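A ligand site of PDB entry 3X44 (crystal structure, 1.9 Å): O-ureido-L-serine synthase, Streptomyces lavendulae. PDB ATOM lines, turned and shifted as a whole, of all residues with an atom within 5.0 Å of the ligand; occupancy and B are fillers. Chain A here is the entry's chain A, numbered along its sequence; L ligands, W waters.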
ATOM      1  N   VAL A  42       4.874 -25.185  17.221  1.00  0.00           N
ATOM      2  CA  VAL A  42       5.677 -24.821  18.378  1.00  0.00           C
ATOM      3  C   VAL A  42       5.741 -23.298  18.581  1.00  0.00           C
ATOM      4  O   VAL A  42       6.040 -22.821  19.677  1.00  0.00           O
ATOM      5  CB  VAL A  42       7.114 -25.387  18.215  1.00  0.00           C
ATOM      6  CG1 VAL A  42       7.775 -24.728  17.046  1.00  0.00           C
ATOM      7  CG2 VAL A  42       7.922 -25.189  19.498  1.00  0.00           C
ATOM      8  N   CYS A  69       8.922 -10.031  12.113  1.00  0.00           N
ATOM      9  CA  CYS A  69       9.341 -10.629  10.839  1.00  0.00           C
ATOM     10  C   CYS A  69       9.308 -12.118  11.139  1.00  0.00           C
ATOM     11  O   CYS A  69       9.916 -12.579  12.105  1.00  0.00           O
ATOM     12  CB  CYS A  69      10.760 -10.212  10.460  1.00  0.00           C
ATOM     13  SG  CYS A  69      11.445 -11.241   9.140  1.00  0.00           S
ATOM     14  N   THR A  70       8.602 -12.882  10.317  1.00  0.00           N
ATOM     15  CA  THR A  70       8.462 -14.306  10.576  1.00  0.00           C
ATOM     16  C   THR A  70       8.554 -15.153   9.314  1.00  0.00           C
ATOM     17  O   THR A  70       8.356 -14.647   8.209  1.00  0.00           O
ATOM     18  CB  THR A  70       7.092 -14.557  11.248  1.00  0.00           C
ATOM     19  OG1 THR A  70       6.872 -15.963  11.389  1.00  0.00           O
ATOM     20  CG2 THR A  70       5.979 -13.981  10.380  1.00  0.00           C
ATOM     21  N   SER A  71       8.864 -16.438   9.483  1.00  0.00           N
ATOM     22  CA  SER A  71       8.904 -17.377   8.361  1.00  0.00           C
ATOM     23  C   SER A  71       7.496 -17.946   8.221  1.00  0.00           C
ATOM     24  O   SER A  71       7.241 -18.795   7.353  1.00  0.00           O
ATOM     25  CB  SER A  71       9.912 -18.516   8.604  1.00  0.00           C
ATOM     26  OG  SER A  71       9.583 -19.281   9.754  1.00  0.00           O
ATOM     27  N   GLY A  72       6.595 -17.500   9.080  1.00  0.00           N
ATOM     28  CA  GLY A  72       5.216 -17.965   9.024  1.00  0.00           C
ATOM     29  C   GLY A  72       4.556 -18.355  10.340  1.00  0.00           C
ATOM     30  O   GLY A  72       3.618 -17.698  10.784  1.00  0.00           O
ATOM     31  N   ASN A  73       5.038 -19.419  10.973  1.00  0.00           N
ATOM     32  CA  ASN A  73       4.458 -19.897  12.228  1.00  0.00           C
ATOM     33  C   ASN A  73       4.389 -18.863  13.339  1.00  0.00           C
ATOM     34  O   ASN A  73       3.384 -18.755  14.031  1.00  0.00           O
ATOM     35  CB  ASN A  73       5.194 -21.158  12.700  1.00  0.00           C
ATOM     36  CG  ASN A  73       4.768 -22.405  11.931  1.00  0.00           C
ATOM     37  OD1 ASN A  73       3.628 -22.516  11.499  1.00  0.00           O
ATOM     38  ND2 ASN A  73       5.700 -23.349  11.764  1.00  0.00           N
ATOM     39  N   VAL A  74       5.443 -18.084  13.530  1.00  0.00           N
ATOM     40  CA  VAL A  74       5.369 -17.099  14.594  1.00  0.00           C
ATOM     41  C   VAL A  74       4.294 -16.071  14.245  1.00  0.00           C
ATOM     42  O   VAL A  74       3.572 -15.603  15.128  1.00  0.00           O
ATOM     43  CB  VAL A  74       6.736 -16.428  14.830  1.00  0.00           C
ATOM     44  CG1 VAL A  74       6.563 -15.122  15.577  1.00  0.00           C
ATOM     45  CG2 VAL A  74       7.616 -17.369  15.640  1.00  0.00           C
ATOM     46  N   GLY A  75       4.175 -15.734  12.969  1.00  0.00           N
ATOM     47  CA  GLY A  75       3.150 -14.804  12.546  1.00  0.00           C
ATOM     48  C   GLY A  75       1.766 -15.359  12.840  1.00  0.00           C
ATOM     49  O   GLY A  75       0.884 -14.654  13.318  1.00  0.00           O
ATOM     50  N   TYR A  97       7.413 -17.860   1.323  1.00  0.00           N
ATOM     51  CA  TYR A  97       6.864 -18.813   2.293  1.00  0.00           C
ATOM     52  C   TYR A  97       5.465 -19.225   1.825  1.00  0.00           C
ATOM     53  O   TYR A  97       4.813 -18.471   1.119  1.00  0.00           O
ATOM     54  CB  TYR A  97       6.853 -18.181   3.696  1.00  0.00           C
ATOM     55  CG  TYR A  97       8.243 -18.089   4.274  1.00  0.00           C
ATOM     56  CD1 TYR A  97       8.923 -16.880   4.345  1.00  0.00           C
ATOM     57  CD2 TYR A  97       8.920 -19.250   4.674  1.00  0.00           C
ATOM     58  CE1 TYR A  97      10.248 -16.817   4.790  1.00  0.00           C
ATOM     59  CE2 TYR A  97      10.236 -19.196   5.115  1.00  0.00           C
ATOM     60  CZ  TYR A  97      10.895 -17.981   5.158  1.00  0.00           C
ATOM     61  OH  TYR A  97      12.202 -17.932   5.577  1.00  0.00           O
ATOM     62  N   ARG A 101       0.425 -19.893   5.098  1.00  0.00           N
ATOM     63  CA  ARG A 101       0.885 -19.009   6.162  1.00  0.00           C
ATOM     64  C   ARG A 101       0.215 -17.649   6.034  1.00  0.00           C
ATOM     65  O   ARG A 101      -0.249 -17.071   7.020  1.00  0.00           O
ATOM     66  CB  ARG A 101       2.407 -18.846   6.089  1.00  0.00           C
ATOM     67  CG  ARG A 101       3.211 -20.000   6.645  1.00  0.00           C
ATOM     68  CD  ARG A 101       4.583 -20.061   5.992  1.00  0.00           C
ATOM     69  NE  ARG A 101       5.532 -20.791   6.825  1.00  0.00           N
ATOM     70  CZ  ARG A 101       5.606 -22.115   6.871  1.00  0.00           C
ATOM     71  NH1 ARG A 101       4.806 -22.859   6.119  1.00  0.00           N
ATOM     72  NH2 ARG A 101       6.479 -22.700   7.687  1.00  0.00           N
ATOM     73  N   SER A 121      15.606 -13.288   6.596  1.00  0.00           N
ATOM     74  CA  SER A 121      15.034 -12.653   7.770  1.00  0.00           C
ATOM     75  C   SER A 121      15.838 -11.417   8.162  1.00  0.00           C
ATOM     76  O   SER A 121      15.361 -10.580   8.925  1.00  0.00           O
ATOM     77  CB  SER A 121      14.989 -13.635   8.931  1.00  0.00           C
ATOM     78  OG  SER A 121      14.030 -14.649   8.685  1.00  0.00           O
ATOM     79  N   GLN A 142      11.766 -11.840  18.084  1.00  0.00           N
ATOM     80  CA  GLN A 142      11.918 -13.263  18.370  1.00  0.00           C
ATOM     81  C   GLN A 142      13.342 -13.818  18.337  1.00  0.00           C
ATOM     82  O   GLN A 142      13.636 -14.812  18.984  1.00  0.00           O
ATOM     83  CB  GLN A 142      11.008 -14.088  17.438  1.00  0.00           C
ATOM     84  CG  GLN A 142      11.342 -14.025  15.942  1.00  0.00           C
ATOM     85  CD  GLN A 142      10.726 -15.189  15.182  1.00  0.00           C
ATOM     86  OE1 GLN A 142      10.601 -16.295  15.708  1.00  0.00           O
ATOM     87  NE2 GLN A 142      10.336 -14.950  13.923  1.00  0.00           N
ATOM     88  N   PHE A 143      14.240 -13.171  17.589  1.00  0.00           N
ATOM     89  CA  PHE A 143      15.618 -13.665  17.512  1.00  0.00           C
ATOM     90  C   PHE A 143      16.511 -13.188  18.640  1.00  0.00           C
ATOM     91  O   PHE A 143      17.653 -13.657  18.775  1.00  0.00           O
ATOM     92  CB  PHE A 143      16.256 -13.244  16.186  1.00  0.00           C
ATOM     93  CG  PHE A 143      15.564 -13.804  14.987  1.00  0.00           C
ATOM     94  CD1 PHE A 143      15.813 -15.115  14.583  1.00  0.00           C
ATOM     95  CD2 PHE A 143      14.680 -13.030  14.240  1.00  0.00           C
ATOM     96  CE1 PHE A 143      15.207 -15.636  13.457  1.00  0.00           C
ATOM     97  CE2 PHE A 143      14.063 -13.549  13.104  1.00  0.00           C
ATOM     98  CZ  PHE A 143      14.322 -14.853  12.713  1.00  0.00           C
ATOM     99  N   ASN A 148      11.836 -15.999  24.694  1.00  0.00           N
ATOM    100  CA  ASN A 148      11.687 -17.081  23.730  1.00  0.00           C
ATOM    101  C   ASN A 148      12.273 -18.365  24.324  1.00  0.00           C
ATOM    102  O   ASN A 148      11.526 -19.270  24.705  1.00  0.00           O
ATOM    103  CB  ASN A 148      12.375 -16.667  22.411  1.00  0.00           C
ATOM    104  CG  ASN A 148      12.473 -17.804  21.404  1.00  0.00           C
ATOM    105  OD1 ASN A 148      12.043 -18.934  21.635  1.00  0.00           O
ATOM    106  ND2 ASN A 148      13.059 -17.493  20.243  1.00  0.00           N
ATOM    107  N   HIS A 152      10.835 -22.202  26.694  1.00  0.00           N
ATOM    108  CA  HIS A 152      11.220 -23.566  26.302  1.00  0.00           C
ATOM    109  C   HIS A 152      11.893 -24.290  27.457  1.00  0.00           C
ATOM    110  O   HIS A 152      11.764 -25.506  27.593  1.00  0.00           O
ATOM    111  CB  HIS A 152      12.148 -23.539  25.088  1.00  0.00           C
ATOM    112  CG  HIS A 152      11.445 -23.192  23.816  1.00  0.00           C
ATOM    113  ND1 HIS A 152      10.533 -24.037  23.213  1.00  0.00           N
ATOM    114  CD2 HIS A 152      11.481 -22.074  23.054  1.00  0.00           C
ATOM    115  CE1 HIS A 152      10.046 -23.464  22.134  1.00  0.00           C
ATOM    116  NE2 HIS A 152      10.609 -22.271  22.014  1.00  0.00           N
ATOM    117  N   GLY A 175      16.128 -28.761  14.691  1.00  0.00           N
ATOM    118  CA  GLY A 175      16.718 -27.831  13.744  1.00  0.00           C
ATOM    119  C   GLY A 175      16.574 -26.501  14.457  1.00  0.00           C
ATOM    120  O   GLY A 175      16.315 -26.476  15.664  1.00  0.00           O
ATOM    121  N   PHE A 176      16.751 -25.393  13.741  1.00  0.00           N
ATOM    122  CA  PHE A 176      16.602 -24.105  14.387  1.00  0.00           C
ATOM    123  C   PHE A 176      16.354 -22.940  13.447  1.00  0.00           C
ATOM    124  O   PHE A 176      16.839 -22.921  12.311  1.00  0.00           O
ATOM    125  CB  PHE A 176      17.797 -23.808  15.285  1.00  0.00           C
ATOM    126  CG  PHE A 176      19.090 -23.588  14.553  1.00  0.00           C
ATOM    127  CD1 PHE A 176      19.365 -22.370  13.954  1.00  0.00           C
ATOM    128  CD2 PHE A 176      20.058 -24.597  14.502  1.00  0.00           C
ATOM    129  CE1 PHE A 176      20.587 -22.143  13.310  1.00  0.00           C
ATOM    130  CE2 PHE A 176      21.281 -24.386  13.874  1.00  0.00           C
ATOM    131  CZ  PHE A 176      21.545 -23.156  13.268  1.00  0.00           C
ATOM    132  N   GLY A 177      15.567 -21.987  13.938  1.00  0.00           N
ATOM    133  CA  GLY A 177      15.261 -20.769  13.214  1.00  0.00           C
ATOM    134  C   GLY A 177      15.803 -19.699  14.146  1.00  0.00           C
ATOM    135  O   GLY A 177      16.851 -19.095  13.884  1.00  0.00           O
ATOM    136  N   THR A 178      15.091 -19.455  15.241  1.00  0.00           N
ATOM    137  CA  THR A 178      15.532 -18.479  16.240  1.00  0.00           C
ATOM    138  C   THR A 178      16.504 -19.157  17.214  1.00  0.00           C
ATOM    139  O   THR A 178      17.281 -18.480  17.903  1.00  0.00           O
ATOM    140  CB  THR A 178      14.350 -17.930  17.042  1.00  0.00           C
ATOM    141  OG1 THR A 178      13.783 -18.974  17.859  1.00  0.00           O
ATOM    142  CG2 THR A 178      13.280 -17.372  16.116  1.00  0.00           C
ATOM    143  N   THR A 179      16.469 -20.492  17.227  1.00  0.00           N
ATOM    144  CA  THR A 179      17.269 -21.351  18.117  1.00  0.00           C
ATOM    145  C   THR A 179      16.708 -21.341  19.535  1.00  0.00           C
ATOM    146  O   THR A 179      17.299 -21.925  20.452  1.00  0.00           O
ATOM    147  CB  THR A 179      18.788 -20.973  18.164  1.00  0.00           C
ATOM    148  OG1 THR A 179      19.023 -19.949  19.140  1.00  0.00           O
ATOM    149  CG2 THR A 179      19.273 -20.536  16.803  1.00  0.00           C
ATOM    150  N   GLY A 180      15.556 -20.720  19.720  1.00  0.00           N
ATOM    151  CA  GLY A 180      14.953 -20.684  21.043  1.00  0.00           C
ATOM    152  C   GLY A 180      14.666 -22.076  21.587  1.00  0.00           C
ATOM    153  O   GLY A 180      14.828 -22.330  22.783  1.00  0.00           O
ATOM    154  N   THR A 181      14.247 -22.984  20.715  1.00  0.00           N
ATOM    155  CA  THR A 181      13.938 -24.349  21.132  1.00  0.00           C
ATOM    156  C   THR A 181      15.221 -25.044  21.529  1.00  0.00           C
ATOM    157  O   THR A 181      15.316 -25.615  22.606  1.00  0.00           O
ATOM    158  CB  THR A 181      13.260 -25.145  19.985  1.00  0.00           C
ATOM    159  OG1 THR A 181      11.943 -24.625  19.764  1.00  0.00           O
ATOM    160  CG2 THR A 181      13.143 -26.610  20.347  1.00  0.00           C
ATOM    161  N   GLN A 220      11.172 -24.458   5.276  1.00  0.00           N
ATOM    162  CA  GLN A 220      10.506 -23.319   5.886  1.00  0.00           C
ATOM    163  C   GLN A 220      10.536 -23.310   7.408  1.00  0.00           C
ATOM    164  O   GLN A 220      10.144 -24.276   8.067  1.00  0.00           O
ATOM    165  CB  GLN A 220       9.049 -23.264   5.387  1.00  0.00           C
ATOM    166  CG  GLN A 220       8.935 -23.440   3.867  1.00  0.00           C
ATOM    167  CD  GLN A 220       7.743 -22.721   3.255  1.00  0.00           C
ATOM    168  OE1 GLN A 220       7.126 -21.866   3.880  1.00  0.00           O
ATOM    169  NE2 GLN A 220       7.404 -23.087   2.026  1.00  0.00           N
ATOM    170  N   GLY A 221      11.008 -22.190   7.958  1.00  0.00           N
ATOM    171  CA  GLY A 221      11.068 -22.068   9.399  1.00  0.00           C
ATOM    172  C   GLY A 221      12.495 -22.126   9.930  1.00  0.00           C
ATOM    173  O   GLY A 221      12.779 -21.591  11.003  1.00  0.00           O
ATOM    174  N   LEU A 222      13.383 -22.755   9.182  1.00  0.00           N
ATOM    175  CA  LEU A 222      14.768 -22.890   9.605  1.00  0.00           C
ATOM    176  C   LEU A 222      15.744 -21.925   8.945  1.00  0.00           C
ATOM    177  O   LEU A 222      15.437 -21.263   7.942  1.00  0.00           O
ATOM    178  CB  LEU A 222      15.297 -24.294   9.324  1.00  0.00           C
ATOM    179  CG  LEU A 222      14.460 -25.506   9.747  1.00  0.00           C
ATOM    180  CD1 LEU A 222      15.218 -26.780   9.397  1.00  0.00           C
ATOM    181  CD2 LEU A 222      14.203 -25.435  11.241  1.00  0.00           C
ATOM    182  N   ALA A 223      16.917 -21.877   9.555  1.00  0.00           N
ATOM    183  CA  ALA A 223      18.062 -21.117   9.100  1.00  0.00           C
ATOM    184  C   ALA A 223      17.905 -19.707   8.549  1.00  0.00           C
ATOM    185  O   ALA A 223      17.849 -19.500   7.336  1.00  0.00           O
ATOM    186  CB  ALA A 223      18.824 -21.961   8.088  1.00  0.00           C
ATOM    187  N   PRO A 224      17.832 -18.712   9.448  1.00  0.00           N
ATOM    188  CA  PRO A 224      17.706 -17.318   8.995  1.00  0.00           C
ATOM    189  C   PRO A 224      19.122 -16.948   8.496  1.00  0.00           C
ATOM    190  O   PRO A 224      20.085 -17.658   8.801  1.00  0.00           O
ATOM    191  CB  PRO A 224      17.322 -16.565  10.254  1.00  0.00           C
ATOM    192  CG  PRO A 224      17.953 -17.370  11.353  1.00  0.00           C
ATOM    193  CD  PRO A 224      17.794 -18.809  10.916  1.00  0.00           C
ATOM    194  N   SER A 265      10.524 -29.116   8.276  1.00  0.00           N
ATOM    195  CA  SER A 265      11.518 -29.135   9.340  1.00  0.00           C
ATOM    196  C   SER A 265      11.303 -30.384  10.191  1.00  0.00           C
ATOM    197  O   SER A 265      12.255 -30.916  10.760  1.00  0.00           O
ATOM    198  CB  SER A 265      11.409 -27.874  10.219  1.00  0.00           C
ATOM    199  OG  SER A 265      10.244 -27.892  11.022  1.00  0.00           O
ATOM    200  N   PRO A 291       8.047 -29.570  14.710  1.00  0.00           N
ATOM    201  CA  PRO A 291       7.553 -28.195  14.898  1.00  0.00           C
ATOM    202  C   PRO A 291       6.124 -27.843  14.501  1.00  0.00           C
ATOM    203  O   PRO A 291       5.474 -27.069  15.206  1.00  0.00           O
ATOM    204  CB  PRO A 291       8.581 -27.341  14.170  1.00  0.00           C
ATOM    205  CG  PRO A 291       9.853 -28.187  14.206  1.00  0.00           C
ATOM    206  CD  PRO A 291       9.314 -29.576  13.950  1.00  0.00           C
ATOM    207  N   ASP A 292       5.631 -28.393  13.406  1.00  0.00           N
ATOM    208  CA  ASP A 292       4.284 -28.045  12.986  1.00  0.00           C
ATOM    209  C   ASP A 292       3.548 -29.105  12.187  1.00  0.00           C
ATOM    210  O   ASP A 292       4.093 -30.168  11.865  1.00  0.00           O
ATOM    211  CB  ASP A 292       4.310 -26.725  12.214  1.00  0.00           C
ATOM    212  CG  ASP A 292       5.041 -26.825  10.869  1.00  0.00           C
ATOM    213  OD1 ASP A 292       5.491 -27.937  10.502  1.00  0.00           O
ATOM    214  OD2 ASP A 292       5.154 -25.777  10.188  1.00  0.00           O
ATOM    215  N   TYR A 297       1.439 -26.873   4.249  1.00  0.00           N
ATOM    216  CA  TYR A 297       2.426 -27.160   3.218  1.00  0.00           C
ATOM    217  C   TYR A 297       1.803 -27.794   1.973  1.00  0.00           C
ATOM    218  O   TYR A 297       2.515 -28.262   1.090  1.00  0.00           O
ATOM    219  CB  TYR A 297       3.500 -28.099   3.784  1.00  0.00           C
ATOM    220  CG  TYR A 297       4.259 -27.498   4.942  1.00  0.00           C
ATOM    221  CD1 TYR A 297       5.460 -26.827   4.720  1.00  0.00           C
ATOM    222  CD2 TYR A 297       3.758 -27.579   6.236  1.00  0.00           C
ATOM    223  CE1 TYR A 297       6.151 -26.244   5.779  1.00  0.00           C
ATOM    224  CE2 TYR A 297       4.440 -26.997   7.295  1.00  0.00           C
ATOM    225  CZ  TYR A 297       5.641 -26.333   7.061  1.00  0.00           C
ATOM    226  OH  TYR A 297       6.324 -25.760   8.117  1.00  0.00           O
HETATM  227  N1  LIG L   1       9.754 -20.376  13.055  1.00  0.00           N
HETATM  228  C1  LIG L   1       9.943 -18.916  13.403  1.00  0.00           C
HETATM  229  C2  LIG L   1      11.362 -18.395  12.994  1.00  0.00           C
HETATM  230  O1  LIG L   1      11.570 -18.573  11.520  1.00  0.00           O
HETATM  231  N2  LIG L   1      12.427 -17.545  10.986  1.00  0.00           N
HETATM  232  C3  LIG L   1      13.565 -17.883  10.334  1.00  0.00           C
HETATM  233  N3  LIG L   1      14.099 -19.104  10.508  1.00  0.00           N
HETATM  234  O2  LIG L   1      14.089 -17.112   9.601  1.00  0.00           O
HETATM  235  C4  LIG L   1       8.863 -18.093  12.665  1.00  0.00           C
HETATM  236  O3  LIG L   1       7.858 -18.640  12.293  1.00  0.00           O
HETATM  237  O4  LIG L   1       9.027 -16.916  12.464  1.00  0.00           O
HETATM  238  C5  LIG L   1       9.350 -24.654  11.915  1.00  0.00           C
HETATM  239  C6  LIG L   1       9.352 -23.253  12.353  1.00  0.00           C
HETATM  240  C7  LIG L   1      10.439 -22.779  13.224  1.00  0.00           C
HETATM  241  C8  LIG L   1      11.476 -23.728  13.640  1.00  0.00           C
HETATM  242  C9  LIG L   1      11.382 -25.114  13.157  1.00  0.00           C
HETATM  243  C10 LIG L   1       8.278 -25.164  11.000  1.00  0.00           C
HETATM  244  C11 LIG L   1      10.597 -21.305  13.545  1.00  0.00           C
HETATM  245  C12 LIG L   1      12.628 -23.311  14.545  1.00  0.00           C
HETATM  246  N4  LIG L   1      10.357 -25.510  12.330  1.00  0.00           N
HETATM  247  O5  LIG L   1       8.338 -22.434  12.020  1.00  0.00           O
HETATM  248  O6  LIG L   1      12.732 -20.798  16.271  1.00  0.00           O
HETATM  249  O7  LIG L   1      12.691 -22.294  18.099  1.00  0.00           O
HETATM  250  O8  LIG L   1      14.427 -22.456  16.485  1.00  0.00           O
HETATM  251  O9  LIG L   1      12.158 -23.108  15.917  1.00  0.00           O
HETATM  252  P1  LIG L   1      13.006 -22.155  16.691  1.00  0.00           P
HETATM  253  O   HOH W   1      11.068 -25.383  17.155  1.00  0.00           O
HETATM  254  O   HOH W   2      11.921 -14.514  10.591  1.00  0.00           O
HETATM  255  O   HOH W   3      11.042 -20.800  19.626  1.00  0.00           O
HETATM  256  O   HOH W   4      15.777 -24.504  17.622  1.00  0.00           O
HETATM  257  O   HOH W   5       7.631 -20.976  10.027  1.00  0.00           O
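The side-chain hydroxyl (OG1) of Thr 181 is in hydrogen-bond range of an oxygen (O7) of the ligand.
The side-chain hydroxyl of Ser 121 lies within hydrogen-bond range of an oxygen (O2) of the ligand.
An oxygen (O8) of the ligand lies within hydrogen-bond range of the backbone NH (N) of Gly 177.
An oxygen (O6) of the ligand lies within hydrogen-bond range of the backbone NH of Thr 178 (2.9 Å).
OG of Ser 71 lies within hydrogen-bond range of O1 of the ligand (2.8 Å).
ND2 of Asn 73 lies within hydrogen-bond range of O5 of the ligand, at 2.8 Å.
The backbone NH of Thr 181 is in hydrogen-bond range of an oxygen (O7) of the ligand, 3.1 Å away.
N of Ser 71 is in hydrogen-bond range of O4 of the ligand.
OG1 of Thr 70 sits at hydrogen-bond distance from O4 of the ligand.
OG of Ser 265 sits at hydrogen-bond distance from N4 of the ligand (2.7 Å).
An oxygen (O3) of the ligand is in hydrogen-bond range of the backbone NH of Val 74, at 2.8 Å.
N of Thr 179 is in hydrogen-bond range of O8 of the ligand (2.9 Å).
O of Gly 221 sits at hydrogen-bond distance from N3 of the ligand (2.9 Å).
The side-chain amide nitrogen (NE2) of Gln 142 is in hydrogen-bond range of an oxygen (O4) of the ligand (2.8 Å).
The backbone NH (N) of Asn 73 lies within hydrogen-bond range of an oxygen (O3) of the ligand, 3.2 Å away.
OG1 of Thr 178 sits at hydrogen-bond distance from O6 of the ligand.
The backbone carbonyl oxygen (O) of Phe 176 sits at hydrogen-bond distance from the backbone NH (N) of Ala 223, at 2.9 Å.
N of Gly 75 sits at hydrogen-bond distance from OG1 of Thr 70, at 3.1 Å.
O of Ser 71 lies within hydrogen-bond range of NE of Arg 101, 2.7 Å away.
The guanidinium group of Arg 101 is in hydrogen-bond range of the side-chain hydroxyl of Tyr 297 (3.1 Å).
OG1 of Thr 178 is in hydrogen-bond range of ND2 of Asn 148, 2.9 Å away.
The side-chain amide nitrogen of Asn 73 is in hydrogen-bond range of the side-chain carboxylate of Asp 292 (2.9 Å).
The side-chain amide nitrogen (NE2) of Gln 142 sits at hydrogen-bond distance from the backbone carbonyl oxygen (O) of Cys 69 (3.0 Å).
The side-chain hydroxyl (OG1) of Thr 70 is in hydrogen-bond range of the backbone NH (N) of Gly 72 (2.8 Å).
Residues that only touch the ligand: Gly 72 (3.6 Å), Phe 143 (3.7 Å), Phe 176 (3.4 Å), Gly 180 (3.6 Å), Gln 220 (3.6 Å), Leu 222 (3.4 Å), Pro 224 (3.3 Å), Pro 291 (3.1 Å), Asp 292 (3.3 Å) and Tyr 297 (3.5 Å).
Hydrophobic or aromatic side chains within 4 Å of the ligand: Val 74, Phe 143, Phe 176, Leu 222, Pro 224 and Pro 291.
The nearest printed residue that does not touch the ligand is Ala 223 (4.1 Å).
Water W5 lies within hydrogen-bond range of O5 of the ligand, OG of Ser 71, NH2 of Arg 101 and N of Asn 73.
Water W3 lies within hydrogen-bond range of O7 of the ligand (2.7 Å), NE2 of His 152 (2.8 Å) and OD1 of Asn 148 (2.9 Å).
Water W4 lies within hydrogen-bond range of O8 of the ligand (2.7 Å) and O of Gly 175 (2.8 Å).
Water W1 bridges O9 of the ligand (2.8 Å) and OG1 of Thr 181 (2.9 Å).
Water W2 lies within hydrogen-bond range of the side-chain hydroxyl (OG) of Ser 121 (2.8 Å), a nitrogen (N2) of the ligand (3.1 Å) and the backbone carbonyl oxygen (O) of Cys 69 (3.2 Å).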
